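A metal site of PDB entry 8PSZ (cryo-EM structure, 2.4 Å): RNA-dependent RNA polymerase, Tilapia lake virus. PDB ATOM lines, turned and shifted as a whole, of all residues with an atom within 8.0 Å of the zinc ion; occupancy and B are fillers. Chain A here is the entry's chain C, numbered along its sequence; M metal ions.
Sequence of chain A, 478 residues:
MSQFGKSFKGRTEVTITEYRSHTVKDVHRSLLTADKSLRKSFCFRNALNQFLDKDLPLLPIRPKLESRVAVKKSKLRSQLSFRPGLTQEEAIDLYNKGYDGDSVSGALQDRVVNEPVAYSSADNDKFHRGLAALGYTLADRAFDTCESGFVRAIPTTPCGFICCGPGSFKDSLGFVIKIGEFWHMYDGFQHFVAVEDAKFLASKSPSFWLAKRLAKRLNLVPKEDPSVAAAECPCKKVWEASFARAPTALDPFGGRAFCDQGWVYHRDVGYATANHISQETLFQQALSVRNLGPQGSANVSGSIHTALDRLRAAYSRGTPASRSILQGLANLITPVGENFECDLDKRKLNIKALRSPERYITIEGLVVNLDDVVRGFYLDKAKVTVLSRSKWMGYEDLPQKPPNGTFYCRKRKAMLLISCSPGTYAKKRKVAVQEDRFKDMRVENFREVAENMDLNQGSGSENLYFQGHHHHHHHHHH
N of Phe 161 sits close to SG of Cys 159 (3.7 Å). NE of Arg 245 is in hydrogen-bond range of O of Cys 163.
Of the 23 residues printed, 4 come within 4 Å of the zinc ion. Along chain A the residues within 4 Å of the zinc ion span positions 146 to 164. The nearest printed residue that does not touch the zinc ion is Lys 170 (4.4 Å).
The zinc ion is bound by the side-chain sulfur of Cys 146, the side-chain sulfur of Cys 159, the side-chain sulfur of Cys 163 and the side-chain sulfur of Cys 164.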
ATOM      1  N   ASP A 144      16.720 -26.266  -1.181  1.00  0.00           N
ATOM      2  CA  ASP A 144      15.905 -27.113  -2.056  1.00  0.00           C
ATOM      3  C   ASP A 144      14.587 -26.427  -2.391  1.00  0.00           C
ATOM      4  O   ASP A 144      13.987 -25.765  -1.537  1.00  0.00           O
ATOM      5  CB  ASP A 144      15.632 -28.463  -1.386  1.00  0.00           C
ATOM      6  CG  ASP A 144      15.258 -28.326   0.075  1.00  0.00           C
ATOM      7  OD1 ASP A 144      15.825 -27.437   0.753  1.00  0.00           O
ATOM      8  OD2 ASP A 144      14.404 -29.103   0.553  1.00  0.00           O
ATOM      9  N   THR A 145      14.139 -26.583  -3.644  1.00  0.00           N
ATOM     10  CA  THR A 145      12.892 -25.960  -4.059  1.00  0.00           C
ATOM     11  C   THR A 145      11.718 -26.408  -3.209  1.00  0.00           C
ATOM     12  O   THR A 145      10.794 -25.631  -2.966  1.00  0.00           O
ATOM     13  CB  THR A 145      12.610 -26.263  -5.532  1.00  0.00           C
ATOM     14  OG1 THR A 145      12.372 -27.668  -5.696  1.00  0.00           O
ATOM     15  CG2 THR A 145      13.781 -25.859  -6.413  1.00  0.00           C
ATOM     16  N   CYS A 146      11.744 -27.662  -2.733  1.00  0.00           N
ATOM     17  CA  CYS A 146      10.654 -28.162  -1.906  1.00  0.00           C
ATOM     18  C   CYS A 146      10.611 -27.446  -0.557  1.00  0.00           C
ATOM     19  O   CYS A 146       9.531 -27.194  -0.023  1.00  0.00           O
ATOM     20  CB  CYS A 146      10.783 -29.664  -1.708  1.00  0.00           C
ATOM     21  SG  CYS A 146       9.988 -30.608  -3.012  1.00  0.00           S
ATOM     22  N   GLU A 147      11.780 -27.122   0.013  1.00  0.00           N
ATOM     23  CA  GLU A 147      11.794 -26.342   1.238  1.00  0.00           C
ATOM     24  C   GLU A 147      11.146 -24.977   1.028  1.00  0.00           C
ATOM     25  O   GLU A 147      10.373 -24.513   1.869  1.00  0.00           O
ATOM     26  CB  GLU A 147      13.236 -26.177   1.735  1.00  0.00           C
ATOM     27  CG  GLU A 147      13.460 -25.005   2.667  1.00  0.00           C
ATOM     28  CD  GLU A 147      14.656 -25.210   3.565  1.00  0.00           C
ATOM     29  OE1 GLU A 147      15.687 -25.717   3.078  1.00  0.00           O
ATOM     30  OE2 GLU A 147      14.572 -24.844   4.759  1.00  0.00           O
ATOM     31  N   SER A 148      11.454 -24.323  -0.094  1.00  0.00           N
ATOM     32  CA  SER A 148      10.851 -23.034  -0.391  1.00  0.00           C
ATOM     33  C   SER A 148       9.353 -23.155  -0.605  1.00  0.00           C
ATOM     34  O   SER A 148       8.577 -22.301  -0.145  1.00  0.00           O
ATOM     35  CB  SER A 148      11.520 -22.412  -1.623  1.00  0.00           C
ATOM     36  OG  SER A 148      10.610 -21.587  -2.334  1.00  0.00           O
ATOM     37  N   GLY A 149       8.910 -24.202  -1.305  1.00  0.00           N
ATOM     38  CA  GLY A 149       7.493 -24.378  -1.591  1.00  0.00           C
ATOM     39  C   GLY A 149       6.671 -24.838  -0.404  1.00  0.00           C
ATOM     40  O   GLY A 149       5.455 -24.618  -0.384  1.00  0.00           O
ATOM     41  N   PHE A 150       7.310 -25.476   0.578  1.00  0.00           N
ATOM     42  CA  PHE A 150       6.578 -25.945   1.744  1.00  0.00           C
ATOM     43  C   PHE A 150       6.056 -24.782   2.582  1.00  0.00           C
ATOM     44  O   PHE A 150       4.968 -24.870   3.169  1.00  0.00           O
ATOM     45  CB  PHE A 150       7.476 -26.849   2.592  1.00  0.00           C
ATOM     46  CG  PHE A 150       6.764 -27.494   3.752  1.00  0.00           C
ATOM     47  CD1 PHE A 150       5.782 -28.439   3.533  1.00  0.00           C
ATOM     48  CD2 PHE A 150       7.091 -27.158   5.053  1.00  0.00           C
ATOM     49  CE1 PHE A 150       5.129 -29.029   4.591  1.00  0.00           C
ATOM     50  CE2 PHE A 150       6.444 -27.749   6.119  1.00  0.00           C
ATOM     51  CZ  PHE A 150       5.459 -28.683   5.891  1.00  0.00           C
ATOM     52  N   PRO A 155       2.512 -22.802  -3.809  1.00  0.00           N
ATOM     53  CA  PRO A 155       3.809 -23.101  -4.420  1.00  0.00           C
ATOM     54  C   PRO A 155       3.785 -22.837  -5.923  1.00  0.00           C
ATOM     55  O   PRO A 155       2.780 -23.054  -6.593  1.00  0.00           O
ATOM     56  CB  PRO A 155       4.020 -24.589  -4.116  1.00  0.00           C
ATOM     57  CG  PRO A 155       3.045 -24.912  -3.029  1.00  0.00           C
ATOM     58  CD  PRO A 155       1.894 -23.994  -3.214  1.00  0.00           C
ATOM     59  N   THR A 157       5.742 -24.328  -8.371  1.00  0.00           N
ATOM     60  CA  THR A 157       5.850 -25.553  -9.164  1.00  0.00           C
ATOM     61  C   THR A 157       5.530 -26.764  -8.292  1.00  0.00           C
ATOM     62  O   THR A 157       6.349 -27.134  -7.434  1.00  0.00           O
ATOM     63  CB  THR A 157       7.247 -25.692  -9.749  1.00  0.00           C
ATOM     64  OG1 THR A 157       8.227 -25.654  -8.704  1.00  0.00           O
ATOM     65  CG2 THR A 157       7.523 -24.572 -10.742  1.00  0.00           C
ATOM     66  N   PRO A 158       4.363 -27.401  -8.455  1.00  0.00           N
ATOM     67  CA  PRO A 158       4.104 -28.620  -7.685  1.00  0.00           C
ATOM     68  C   PRO A 158       5.105 -29.705  -8.015  1.00  0.00           C
ATOM     69  O   PRO A 158       5.510 -29.866  -9.171  1.00  0.00           O
ATOM     70  CB  PRO A 158       2.677 -29.015  -8.104  1.00  0.00           C
ATOM     71  CG  PRO A 158       2.456 -28.331  -9.408  1.00  0.00           C
ATOM     72  CD  PRO A 158       3.238 -27.059  -9.335  1.00  0.00           C
ATOM     73  N   CYS A 159       5.508 -30.463  -6.995  1.00  0.00           N
ATOM     74  CA  CYS A 159       6.446 -31.564  -7.150  1.00  0.00           C
ATOM     75  C   CYS A 159       5.775 -32.927  -7.132  1.00  0.00           C
ATOM     76  O   CYS A 159       6.471 -33.949  -7.172  1.00  0.00           O
ATOM     77  CB  CYS A 159       7.519 -31.501  -6.071  1.00  0.00           C
ATOM     78  SG  CYS A 159       6.934 -31.911  -4.407  1.00  0.00           S
ATOM     79  N   GLY A 160       4.447 -32.973  -7.069  1.00  0.00           N
ATOM     80  CA  GLY A 160       3.745 -34.233  -6.958  1.00  0.00           C
ATOM     81  C   GLY A 160       3.738 -34.824  -5.562  1.00  0.00           C
ATOM     82  O   GLY A 160       3.658 -36.042  -5.421  1.00  0.00           O
ATOM     83  N   PHE A 161       3.828 -33.991  -4.530  1.00  0.00           N
ATOM     84  CA  PHE A 161       3.844 -34.475  -3.159  1.00  0.00           C
ATOM     85  C   PHE A 161       3.200 -33.434  -2.246  1.00  0.00           C
ATOM     86  O   PHE A 161       2.894 -32.315  -2.664  1.00  0.00           O
ATOM     87  CB  PHE A 161       5.262 -34.803  -2.714  1.00  0.00           C
ATOM     88  CG  PHE A 161       5.862 -35.982  -3.437  1.00  0.00           C
ATOM     89  CD1 PHE A 161       5.517 -37.274  -3.086  1.00  0.00           C
ATOM     90  CD2 PHE A 161       6.761 -35.788  -4.472  1.00  0.00           C
ATOM     91  CE1 PHE A 161       6.059 -38.355  -3.746  1.00  0.00           C
ATOM     92  CE2 PHE A 161       7.310 -36.871  -5.138  1.00  0.00           C
ATOM     93  CZ  PHE A 161       6.957 -38.158  -4.768  1.00  0.00           C
ATOM     94  N   ILE A 162       3.004 -33.827  -0.988  1.00  0.00           N
ATOM     95  CA  ILE A 162       2.187 -33.025  -0.068  1.00  0.00           C
ATOM     96  C   ILE A 162       2.818 -31.666   0.190  1.00  0.00           C
ATOM     97  O   ILE A 162       2.106 -30.670   0.353  1.00  0.00           O
ATOM     98  CB  ILE A 162       1.952 -33.802   1.246  1.00  0.00           C
ATOM     99  CG1 ILE A 162       0.909 -33.099   2.109  1.00  0.00           C
ATOM    100  CG2 ILE A 162       3.254 -33.979   2.013  1.00  0.00           C
ATOM    101  CD1 ILE A 162      -0.509 -33.498   1.798  1.00  0.00           C
ATOM    102  N   CYS A 163       4.150 -31.591   0.231  1.00  0.00           N
ATOM    103  CA  CYS A 163       4.789 -30.331   0.594  1.00  0.00           C
ATOM    104  C   CYS A 163       4.440 -29.229  -0.397  1.00  0.00           C
ATOM    105  O   CYS A 163       4.228 -28.080  -0.011  1.00  0.00           O
ATOM    106  CB  CYS A 163       6.308 -30.504   0.664  1.00  0.00           C
ATOM    107  SG  CYS A 163       7.017 -31.338  -0.767  1.00  0.00           S
ATOM    108  N   CYS A 164       4.393 -29.572  -1.689  1.00  0.00           N
ATOM    109  CA  CYS A 164       4.317 -28.575  -2.746  1.00  0.00           C
ATOM    110  C   CYS A 164       2.967 -28.599  -3.459  1.00  0.00           C
ATOM    111  O   CYS A 164       2.787 -27.914  -4.474  1.00  0.00           O
ATOM    112  CB  CYS A 164       5.429 -28.808  -3.765  1.00  0.00           C
ATOM    113  SG  CYS A 164       7.050 -28.174  -3.280  1.00  0.00           S
ATOM    114  N   GLY A 165       2.003 -29.357  -2.942  1.00  0.00           N
ATOM    115  CA  GLY A 165       0.715 -29.510  -3.570  1.00  0.00           C
ATOM    116  C   GLY A 165       0.050 -30.783  -3.105  1.00  0.00           C
ATOM    117  O   GLY A 165       0.529 -31.446  -2.169  1.00  0.00           O
ATOM    118  N   SER A 168       1.409 -37.443  -1.905  1.00  0.00           N
ATOM    119  CA  SER A 168       1.772 -38.284  -0.778  1.00  0.00           C
ATOM    120  C   SER A 168       2.966 -37.679  -0.038  1.00  0.00           C
ATOM    121  O   SER A 168       3.351 -36.527  -0.276  1.00  0.00           O
ATOM    122  CB  SER A 168       2.067 -39.701  -1.262  1.00  0.00           C
ATOM    123  OG  SER A 168       1.849 -40.645  -0.221  1.00  0.00           O
ATOM    124  N   LYS A 170       6.805 -37.246   1.105  1.00  0.00           N
ATOM    125  CA  LYS A 170       8.199 -37.420   0.709  1.00  0.00           C
ATOM    126  C   LYS A 170       9.043 -37.875   1.894  1.00  0.00           C
ATOM    127  O   LYS A 170       8.569 -37.967   3.023  1.00  0.00           O
ATOM    128  CB  LYS A 170       8.758 -36.122   0.140  1.00  0.00           C
ATOM    129  CG  LYS A 170       8.631 -35.994  -1.370  1.00  0.00           C
ATOM    130  CD  LYS A 170       8.704 -34.538  -1.826  1.00  0.00           C
ATOM    131  CE  LYS A 170      10.132 -34.125  -2.137  1.00  0.00           C
ATOM    132  NZ  LYS A 170      11.050 -34.310  -0.978  1.00  0.00           N
ATOM    133  N   SER A 172      11.798 -36.303   3.197  1.00  0.00           N
ATOM    134  CA  SER A 172      12.123 -35.198   4.102  1.00  0.00           C
ATOM    135  C   SER A 172      10.937 -34.748   4.933  1.00  0.00           C
ATOM    136  O   SER A 172      11.120 -33.984   5.881  1.00  0.00           O
ATOM    137  CB  SER A 172      12.664 -34.022   3.296  1.00  0.00           C
ATOM    138  OG  SER A 172      11.978 -33.887   2.061  1.00  0.00           O
ATOM    139  N   LEU A 173       9.723 -35.193   4.609  1.00  0.00           N
ATOM    140  CA  LEU A 173       8.521 -34.791   5.315  1.00  0.00           C
ATOM    141  C   LEU A 173       8.138 -35.862   6.337  1.00  0.00           C
ATOM    142  O   LEU A 173       8.142 -37.053   6.018  1.00  0.00           O
ATOM    143  CB  LEU A 173       7.361 -34.573   4.340  1.00  0.00           C
ATOM    144  CG  LEU A 173       7.672 -33.707   3.122  1.00  0.00           C
ATOM    145  CD1 LEU A 173       6.495 -33.703   2.163  1.00  0.00           C
ATOM    146  CD2 LEU A 173       8.003 -32.286   3.563  1.00  0.00           C
ATOM    147  N   ARG A 245      -3.486 -30.394  -0.214  1.00  0.00           N
ATOM    148  CA  ARG A 245      -2.693 -29.377   0.475  1.00  0.00           C
ATOM    149  C   ARG A 245      -3.482 -28.075   0.468  1.00  0.00           C
ATOM    150  O   ARG A 245      -3.644 -27.440  -0.582  1.00  0.00           O
ATOM    151  CB  ARG A 245      -1.334 -29.195  -0.194  1.00  0.00           C
ATOM    152  CG  ARG A 245      -0.423 -28.185   0.491  1.00  0.00           C
ATOM    153  CD  ARG A 245       0.754 -27.857  -0.395  1.00  0.00           C
ATOM    154  NE  ARG A 245       1.801 -27.103   0.281  1.00  0.00           N
ATOM    155  CZ  ARG A 245       1.825 -25.781   0.394  1.00  0.00           C
ATOM    156  NH1 ARG A 245       0.824 -25.030  -0.052  1.00  0.00           N
ATOM    157  NH2 ARG A 245       2.883 -25.200   0.954  1.00  0.00           N
ATOM    158  N   HIS A 266       8.422 -30.393   7.969  1.00  0.00           N
ATOM    159  CA  HIS A 266       9.610 -30.508   7.128  1.00  0.00           C
ATOM    160  C   HIS A 266      10.840 -30.377   8.005  1.00  0.00           C
ATOM    161  O   HIS A 266      10.909 -29.489   8.857  1.00  0.00           O
ATOM    162  CB  HIS A 266       9.615 -29.435   6.034  1.00  0.00           C
ATOM    163  CG  HIS A 266      10.621 -29.670   4.956  1.00  0.00           C
ATOM    164  ND1 HIS A 266      11.964 -29.417   5.135  1.00  0.00           N
ATOM    165  CD2 HIS A 266      10.496 -30.133   3.693  1.00  0.00           C
ATOM    166  CE1 HIS A 266      12.614 -29.707   4.021  1.00  0.00           C
ATOM    167  NE2 HIS A 266      11.744 -30.147   3.131  1.00  0.00           N
HETATM  168 ZN    ZN M   1       7.683 -30.386  -2.802  1.00  0.00          ZN
